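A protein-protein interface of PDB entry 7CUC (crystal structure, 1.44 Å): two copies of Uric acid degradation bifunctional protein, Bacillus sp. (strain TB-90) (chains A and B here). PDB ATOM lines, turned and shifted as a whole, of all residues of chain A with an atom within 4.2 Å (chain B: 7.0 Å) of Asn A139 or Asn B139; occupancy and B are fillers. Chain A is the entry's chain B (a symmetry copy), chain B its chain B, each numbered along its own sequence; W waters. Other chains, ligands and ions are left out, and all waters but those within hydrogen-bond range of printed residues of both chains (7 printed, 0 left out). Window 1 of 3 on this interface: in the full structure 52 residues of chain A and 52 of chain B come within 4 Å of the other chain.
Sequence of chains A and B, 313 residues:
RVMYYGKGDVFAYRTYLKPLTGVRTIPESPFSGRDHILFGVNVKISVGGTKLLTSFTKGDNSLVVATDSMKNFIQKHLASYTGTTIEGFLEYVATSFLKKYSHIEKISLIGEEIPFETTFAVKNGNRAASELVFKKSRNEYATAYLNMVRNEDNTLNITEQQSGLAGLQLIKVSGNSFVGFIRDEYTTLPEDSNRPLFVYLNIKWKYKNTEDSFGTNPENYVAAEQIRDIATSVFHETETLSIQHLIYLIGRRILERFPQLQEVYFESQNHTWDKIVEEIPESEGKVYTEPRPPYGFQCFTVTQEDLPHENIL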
ATOM      1  N   LYS A 136       7.615   1.584  30.638  1.00  0.00           N
ATOM      2  CA  LYS A 136       6.696   2.402  29.861  1.00  0.00           C
ATOM      3  C   LYS A 136       7.349   3.752  29.588  1.00  0.00           C
ATOM      4  O   LYS A 136       7.917   4.373  30.492  1.00  0.00           O
ATOM      5  CB  LYS A 136       5.371   2.587  30.602  1.00  0.00           C
ATOM      6  CG  LYS A 136       4.330   3.373  29.796  1.00  0.00           C
ATOM      7  CD  LYS A 136       2.916   3.239  30.383  1.00  0.00           C
ATOM      8  CE  LYS A 136       1.850   3.942  29.542  1.00  0.00           C
ATOM      9  NZ  LYS A 136       2.407   4.750  28.439  1.00  0.00           N
ATOM     10  N   SER A 137       7.334   4.179  28.332  1.00  0.00           N
ATOM     11  CA  SER A 137       7.885   5.472  27.968  1.00  0.00           C
ATOM     12  C   SER A 137       6.815   6.512  27.642  1.00  0.00           C
ATOM     13  O   SER A 137       5.849   6.225  26.931  1.00  0.00           O
ATOM     14  CB  SER A 137       8.855   5.358  26.790  1.00  0.00           C
ATOM     15  OG  SER A 137       9.323   6.646  26.418  1.00  0.00           O
ATOM     16  N   ARG A 138       7.048   7.737  28.114  1.00  0.00           N
ATOM     17  CA  ARG A 138       6.184   8.877  27.879  1.00  0.00           C
ATOM     18  C   ARG A 138       6.848   9.831  26.896  1.00  0.00           C
ATOM     19  O   ARG A 138       6.459  10.993  26.800  1.00  0.00           O
ATOM     20  CB  ARG A 138       5.822   9.554  29.197  1.00  0.00           C
ATOM     21  CG  ARG A 138       4.827   8.732  30.020  1.00  0.00           C
ATOM     22  CD  ARG A 138       5.497   7.697  30.896  1.00  0.00           C
ATOM     23  NE  ARG A 138       6.020   8.311  32.115  1.00  0.00           N
ATOM     24  CZ  ARG A 138       6.913   7.754  32.916  1.00  0.00           C
ATOM     25  NH1 ARG A 138       7.372   6.545  32.641  1.00  0.00           N
ATOM     26  NH2 ARG A 138       7.319   8.402  34.001  1.00  0.00           N
ATOM     27  N   ASN A 139       7.852   9.347  26.173  1.00  0.00           N
ATOM     28  CA  ASN A 139       8.523  10.151  25.164  1.00  0.00           C
ATOM     29  C   ASN A 139       7.914   9.944  23.786  1.00  0.00           C
ATOM     30  O   ASN A 139       6.698   9.792  23.676  1.00  0.00           O
ATOM     31  CB  ASN A 139      10.034   9.900  25.229  1.00  0.00           C
ATOM     32  CG  ASN A 139      10.594  10.257  26.597  1.00  0.00           C
ATOM     33  OD1 ASN A 139      10.068  11.154  27.261  1.00  0.00           O
ATOM     34  ND2 ASN A 139      11.673   9.611  27.005  1.00  0.00           N
ATOM     35  N   GLU A 140       8.705   9.962  22.729  1.00  0.00           N
ATOM     36  CA  GLU A 140       8.125   9.939  21.395  1.00  0.00           C
ATOM     37  C   GLU A 140       7.528   8.568  21.050  1.00  0.00           C
ATOM     38  O   GLU A 140       7.851   7.543  21.653  1.00  0.00           O
ATOM     39  CB  GLU A 140       9.170  10.323  20.351  1.00  0.00           C
ATOM     40  CG  GLU A 140      10.326   9.361  20.165  1.00  0.00           C
ATOM     41  CD  GLU A 140      11.409   9.457  21.222  1.00  0.00           C
ATOM     42  OE1 GLU A 140      11.311  10.277  22.167  1.00  0.00           O
ATOM     43  OE2 GLU A 140      12.416   8.738  21.054  1.00  0.00           O
ATOM     44  N   TYR A 141       6.634   8.572  20.070  1.00  0.00           N
ATOM     45  CA  TYR A 141       5.897   7.379  19.710  1.00  0.00           C
ATOM     46  C   TYR A 141       5.471   7.472  18.256  1.00  0.00           C
ATOM     47  O   TYR A 141       5.326   8.565  17.695  1.00  0.00           O
ATOM     48  CB  TYR A 141       4.680   7.211  20.633  1.00  0.00           C
ATOM     49  CG  TYR A 141       3.737   8.408  20.677  1.00  0.00           C
ATOM     50  CD1 TYR A 141       3.955   9.473  21.560  1.00  0.00           C
ATOM     51  CD2 TYR A 141       2.638   8.485  19.827  1.00  0.00           C
ATOM     52  CE1 TYR A 141       3.102  10.563  21.589  1.00  0.00           C
ATOM     53  CE2 TYR A 141       1.786   9.574  19.863  1.00  0.00           C
ATOM     54  CZ  TYR A 141       2.027  10.607  20.731  1.00  0.00           C
ATOM     55  OH  TYR A 141       1.181  11.675  20.732  1.00  0.00           O
ATOM     56  N   GLY A 167       5.780  13.614  19.417  1.00  0.00           N
ATOM     57  CA  GLY A 167       6.321  13.787  20.759  1.00  0.00           C
ATOM     58  C   GLY A 167       7.836  13.803  20.875  1.00  0.00           C
ATOM     59  O   GLY A 167       8.365  13.567  21.963  1.00  0.00           O
ATOM     60  N   GLU B 113      15.588  16.261  39.151  1.00  0.00           N
ATOM     61  CA  GLU B 113      16.323  16.261  37.897  1.00  0.00           C
ATOM     62  C   GLU B 113      15.346  16.436  36.738  1.00  0.00           C
ATOM     63  O   GLU B 113      14.229  15.888  36.743  1.00  0.00           O
ATOM     64  CB  GLU B 113      17.034  14.918  37.762  1.00  0.00           C
ATOM     65  CG  GLU B 113      17.693  14.677  36.415  1.00  0.00           C
ATOM     66  CD  GLU B 113      18.167  13.231  36.195  1.00  0.00           C
ATOM     67  OE1 GLU B 113      17.650  12.279  36.808  1.00  0.00           O
ATOM     68  OE2 GLU B 113      19.096  13.030  35.374  1.00  0.00           O
ATOM     69  N   PRO B 115      15.522  15.196  33.229  1.00  0.00           N
ATOM     70  CA  PRO B 115      16.459  14.318  32.527  1.00  0.00           C
ATOM     71  C   PRO B 115      16.477  14.485  31.009  1.00  0.00           C
ATOM     72  O   PRO B 115      15.476  14.800  30.370  1.00  0.00           O
ATOM     73  CB  PRO B 115      15.978  12.906  32.908  1.00  0.00           C
ATOM     74  CG  PRO B 115      14.494  13.063  33.035  1.00  0.00           C
ATOM     75  CD  PRO B 115      14.300  14.461  33.630  1.00  0.00           C
ATOM     76  N   GLU B 117      18.380  12.547  27.443  1.00  0.00           N
ATOM     77  CA  GLU B 117      18.998  11.355  26.892  1.00  0.00           C
ATOM     78  C   GLU B 117      19.868  11.664  25.680  1.00  0.00           C
ATOM     79  O   GLU B 117      19.626  12.617  24.934  1.00  0.00           O
ATOM     80  CB  GLU B 117      17.918  10.328  26.539  1.00  0.00           C
ATOM     81  CG  GLU B 117      17.204   9.818  27.786  1.00  0.00           C
ATOM     82  CD  GLU B 117      16.102   8.841  27.543  1.00  0.00           C
ATOM     83  OE1 GLU B 117      15.760   8.563  26.368  1.00  0.00           O
ATOM     84  OE2 GLU B 117      15.566   8.362  28.565  1.00  0.00           O
ATOM     85  N   LYS B 135      17.775  14.646  23.950  1.00  0.00           N
ATOM     86  CA  LYS B 135      16.344  14.384  23.925  1.00  0.00           C
ATOM     87  C   LYS B 135      15.809  14.582  25.341  1.00  0.00           C
ATOM     88  O   LYS B 135      16.323  13.990  26.293  1.00  0.00           O
ATOM     89  CB  LYS B 135      16.079  12.968  23.415  1.00  0.00           C
ATOM     90  CG  LYS B 135      14.617  12.690  23.175  1.00  0.00           C
ATOM     91  CD  LYS B 135      14.401  11.282  22.613  1.00  0.00           C
ATOM     92  CE  LYS B 135      14.367  10.258  23.733  1.00  0.00           C
ATOM     93  NZ  LYS B 135      14.088   8.878  23.247  1.00  0.00           N
ATOM     94  N   LYS B 136      14.814  15.452  25.482  1.00  0.00           N
ATOM     95  CA  LYS B 136      14.180  15.634  26.779  1.00  0.00           C
ATOM     96  C   LYS B 136      13.364  14.388  27.107  1.00  0.00           C
ATOM     97  O   LYS B 136      12.620  13.881  26.262  1.00  0.00           O
ATOM     98  CB  LYS B 136      13.288  16.876  26.781  1.00  0.00           C
ATOM     99  CG  LYS B 136      12.656  17.166  28.148  1.00  0.00           C
ATOM    100  CD  LYS B 136      12.073  18.586  28.231  1.00  0.00           C
ATOM    101  CE  LYS B 136      11.519  18.926  29.615  1.00  0.00           C
ATOM    102  NZ  LYS B 136      11.495  17.775  30.539  1.00  0.00           N
ATOM    103  N   SER B 137      13.551  13.851  28.305  1.00  0.00           N
ATOM    104  CA  SER B 137      12.791  12.692  28.739  1.00  0.00           C
ATOM    105  C   SER B 137      11.726  13.027  29.781  1.00  0.00           C
ATOM    106  O   SER B 137      11.981  13.772  30.730  1.00  0.00           O
ATOM    107  CB  SER B 137      13.705  11.594  29.286  1.00  0.00           C
ATOM    108  OG  SER B 137      12.928  10.505  29.761  1.00  0.00           O
ATOM    109  N   ARG B 138      10.557  12.404  29.622  1.00  0.00           N
ATOM    110  CA  ARG B 138       9.432  12.545  30.524  1.00  0.00           C
ATOM    111  C   ARG B 138       9.265  11.271  31.341  1.00  0.00           C
ATOM    112  O   ARG B 138       8.207  11.040  31.922  1.00  0.00           O
ATOM    113  CB  ARG B 138       8.170  12.913  29.751  1.00  0.00           C
ATOM    114  CG  ARG B 138       8.193  14.361  29.254  1.00  0.00           C
ATOM    115  CD  ARG B 138       8.889  14.516  27.920  1.00  0.00           C
ATOM    116  NE  ARG B 138       7.998  14.139  26.824  1.00  0.00           N
ATOM    117  CZ  ARG B 138       8.393  13.867  25.592  1.00  0.00           C
ATOM    118  NH1 ARG B 138       9.675  13.956  25.283  1.00  0.00           N
ATOM    119  NH2 ARG B 138       7.496  13.536  24.671  1.00  0.00           N
ATOM    120  N   ASN B 139      10.302  10.441  31.380  1.00  0.00           N
ATOM    121  CA  ASN B 139      10.275   9.222  32.173  1.00  0.00           C
ATOM    122  C   ASN B 139      10.866   9.441  33.557  1.00  0.00           C
ATOM    123  O   ASN B 139      10.666  10.504  34.142  1.00  0.00           O
ATOM    124  CB  ASN B 139      10.926   8.081  31.383  1.00  0.00           C
ATOM    125  CG  ASN B 139      10.198   7.833  30.071  1.00  0.00           C
ATOM    126  OD1 ASN B 139       8.987   8.054  29.990  1.00  0.00           O
ATOM    127  ND2 ASN B 139      10.898   7.333  29.067  1.00  0.00           N
ATOM    128  N   GLU B 140      11.560   8.467  34.117  1.00  0.00           N
ATOM    129  CA  GLU B 140      11.986   8.590  35.502  1.00  0.00           C
ATOM    130  C   GLU B 140      13.109   9.622  35.670  1.00  0.00           C
ATOM    131  O   GLU B 140      13.808   9.989  34.725  1.00  0.00           O
ATOM    132  CB  GLU B 140      12.444   7.238  36.042  1.00  0.00           C
ATOM    133  CG  GLU B 140      13.696   6.650  35.421  1.00  0.00           C
ATOM    134  CD  GLU B 140      13.486   5.992  34.071  1.00  0.00           C
ATOM    135  OE1 GLU B 140      12.349   5.967  33.540  1.00  0.00           O
ATOM    136  OE2 GLU B 140      14.478   5.424  33.569  1.00  0.00           O
ATOM    137  N   TYR B 141      13.258  10.097  36.900  1.00  0.00           N
ATOM    138  CA  TYR B 141      14.193  11.162  37.194  1.00  0.00           C
ATOM    139  C   TYR B 141      14.622  11.068  38.647  1.00  0.00           C
ATOM    140  O   TYR B 141      13.901  10.533  39.497  1.00  0.00           O
ATOM    141  CB  TYR B 141      13.553  12.526  36.893  1.00  0.00           C
ATOM    142  CG  TYR B 141      12.232  12.787  37.608  1.00  0.00           C
ATOM    143  CD1 TYR B 141      11.014  12.366  37.061  1.00  0.00           C
ATOM    144  CD2 TYR B 141      12.199  13.438  38.837  1.00  0.00           C
ATOM    145  CE1 TYR B 141       9.817  12.595  37.718  1.00  0.00           C
ATOM    146  CE2 TYR B 141      11.001  13.669  39.489  1.00  0.00           C
ATOM    147  CZ  TYR B 141       9.824  13.238  38.935  1.00  0.00           C
ATOM    148  OH  TYR B 141       8.660  13.464  39.607  1.00  0.00           O
ATOM    149  N   ALA B 166      12.101   8.926  40.983  1.00  0.00           N
ATOM    150  CA  ALA B 166      10.670   9.106  40.832  1.00  0.00           C
ATOM    151  C   ALA B 166      10.277   8.735  39.415  1.00  0.00           C
ATOM    152  O   ALA B 166      11.073   8.887  38.478  1.00  0.00           O
ATOM    153  CB  ALA B 166      10.286  10.558  41.085  1.00  0.00           C
ATOM    154  N   GLY B 167       9.028   8.328  39.257  1.00  0.00           N
ATOM    155  CA  GLY B 167       8.461   8.172  37.924  1.00  0.00           C
ATOM    156  C   GLY B 167       8.866   6.920  37.165  1.00  0.00           C
ATOM    157  O   GLY B 167       8.751   6.889  35.937  1.00  0.00           O
ATOM    158  N   LEU B 168       9.291   5.868  37.857  1.00  0.00           N
ATOM    159  CA  LEU B 168       9.679   4.620  37.209  1.00  0.00           C
ATOM    160  C   LEU B 168       8.425   3.784  37.000  1.00  0.00           C
ATOM    161  O   LEU B 168       7.681   3.527  37.956  1.00  0.00           O
ATOM    162  CB  LEU B 168      10.677   3.870  38.087  1.00  0.00           C
ATOM    163  CG  LEU B 168      11.276   2.617  37.449  1.00  0.00           C
ATOM    164  CD1 LEU B 168      11.975   2.922  36.141  1.00  0.00           C
ATOM    165  CD2 LEU B 168      12.229   1.919  38.414  1.00  0.00           C
ATOM    166  N   GLN B 169       8.163   3.398  35.755  1.00  0.00           N
ATOM    167  CA  GLN B 169       6.966   2.657  35.396  1.00  0.00           C
ATOM    168  C   GLN B 169       7.402   1.371  34.701  1.00  0.00           C
ATOM    169  O   GLN B 169       7.947   1.412  33.586  1.00  0.00           O
ATOM    170  CB  GLN B 169       6.068   3.504  34.497  1.00  0.00           C
ATOM    171  CG  GLN B 169       5.593   4.785  35.128  1.00  0.00           C
ATOM    172  CD  GLN B 169       4.589   5.525  34.300  1.00  0.00           C
ATOM    173  OE1 GLN B 169       4.177   5.066  33.243  1.00  0.00           O
ATOM    174  NE2 GLN B 169       4.185   6.714  34.782  1.00  0.00           N
HETATM  175  O   HOH W   1       4.859  11.971  24.214  1.00  0.00           O
HETATM  176  O   HOH W   2       5.068  13.044  27.741  1.00  0.00           O
HETATM  177  O   HOH W   3       5.633  11.542  32.311  1.00  0.00           O
HETATM  178  O   HOH W   4       9.585   4.865  33.619  1.00  0.00           O
HETATM  179  O   HOH W   5       8.021  11.211  35.106  1.00  0.00           O
HETATM  180  O   HOH W   6      11.348  13.134  23.002  1.00  0.00           O
HETATM  181  O   HOH W   7      13.289   7.608  25.709  1.00  0.00           O
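Among the printed residues, merely in contact across the chains: Arg A138 with Gln B169 (3.4 Å), Lys A136 with Asn B139 (3.9 Å) and Asn A139 with Lys B136 (3.9 Å).
The side-chain carboxylate of Glu A140 is in salt-bridge range of the side-chain amino group of Lys B135.
ND2 of Asn A139 lies within hydrogen-bond range of OG of Ser B137 (3.2 Å).
O of Arg B138 sits at hydrogen-bond distance from NH2 of Arg A138 (3.5 Å).
N of Arg B138 lies within hydrogen-bond range of OD1 of Asn A139, 2.7 Å away.
The guanidinium group (NH2) of Arg B138 sits at hydrogen-bond distance from the backbone carbonyl oxygen (O) of Gly A167 (2.8 Å).
ND2 of Asn B139 sits at hydrogen-bond distance from OG of Ser A137.
The backbone NH (N) of Arg A138 lies within hydrogen-bond range of the side-chain amide oxygen (OD1) of Asn B139, 2.7 Å away.
The side-chain amide nitrogen (ND2) of Asn B139 sits close to the side-chain amide nitrogen (ND2) of Asn A139, at 3.2 Å.
The backbone carbonyl oxygen (O) of Gly B167 sits at hydrogen-bond distance from the guanidinium group (NH2) of Arg A138 (2.8 Å).
O of Gln B169 lies within hydrogen-bond range of N of Lys A136.
The backbone carbonyl oxygen (O) of Pro B115 is in hydrogen-bond range of the backbone NH (N) of Ser B137 (3.0 Å).
The side-chain carboxylate (OE1) of Glu B117 is in salt-bridge range of the side-chain amino group (NZ) of Lys B135 (3.6 Å).
The backbone carbonyl oxygen of Lys B136 lies within hydrogen-bond range of the guanidinium group of Arg B138 (3.1 Å).
The side-chain hydroxyl (OG) of Ser B137 is in hydrogen-bond range of the backbone NH (N) of Asn B139.
The backbone carbonyl oxygen (O) of Lys A136 lies within hydrogen-bond range of the guanidinium group (NH1) of Arg A138.
OG of Ser A137 lies within hydrogen-bond range of N of Asn A139, 3.1 Å away.
Printed residues of chain B within 4 Å of Asn A139: Lys B136 (3.9 Å), Ser B137 (3.2 Å), Arg B138 (2.7 Å) and Asn B139 (3.2 Å).
Printed residues of chain A within 4 Å of Asn B139: Lys A136, Ser A137, Arg A138 and Asn A139.
Of the printed residues of chain A, Gly B167 touches Arg A138 (2.8 Å).
Printed residues of chain A within 4 Å of Lys B135: Glu A140.
Of the printed residues of chain B, Lys A136 touches Asn B139 and Gln B169.
Printed residues of chain A within 4 Å of Arg B138: Arg A138 (3.5 Å), Asn A139 (2.7 Å) and Gly A167 (2.8 Å).
Of the printed residues of chain B, Gly A167 touches Arg B138.
Glu B117 touches none of the printed residues of chain A.
Glu B140 touches none of the printed residues of chain A.
The nearest printed residue of chain B that does not touch Asn A139 is Glu B117 (4.3 Å).
Among the printed residues, 13 pairs touch across the chains.
Among the printed residues, Asp or Glu carboxylates within 4 Å of a Lys or Arg side-chain nitrogen of the other chain: Glu A140 with Lys B135.
Water W3 lies within hydrogen-bond range of the backbone carbonyl oxygen (O) of Arg B138 and the guanidinium group (NE) of Arg A138.
Water W7 lies within hydrogen-bond range of the side-chain carboxylate (OE1) of Glu B117, the side-chain amide nitrogen (ND2) of Asn A139 and the side-chain amino group (NZ) of Lys B135.
Water W1 lies within hydrogen-bond range of the backbone carbonyl oxygen of Asn A139 (2.9 Å), the guanidinium group of Arg B138 (3.1 Å) and the backbone carbonyl oxygen of Arg A138 (3.2 Å).
Water W5 lies within hydrogen-bond range of the backbone carbonyl oxygen of Asn B139, the guanidinium group of Arg A138 and the backbone carbonyl oxygen of Arg B138.
Water W4 lies within hydrogen-bond range of NH1 of Arg A138 (2.9 Å), N of Gln B169 (3.0 Å), OE1 of Glu B140 (3.0 Å) and O of Gly B167 (3.2 Å).
Water W6 lies within hydrogen-bond range of NH1 of Arg B138 (2.9 Å), OE1 of Glu A140 (3.0 Å) and O of Gly A167 (3.2 Å).
Lys A136 touches Asn B139, and with the chains exchanged Asn A139 touches Lys B136.
Arg A138 touches its own counterpart, Arg B138.
Arg A138 touches Asn B139, and with the chains exchanged Asn A139 touches Arg B138.
Asn B139 touches its own counterpart, Asn A139.
Of the 13 pairs that touch across the chains among the printed residues, 10 have their exchanged pair printed and touching as well.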
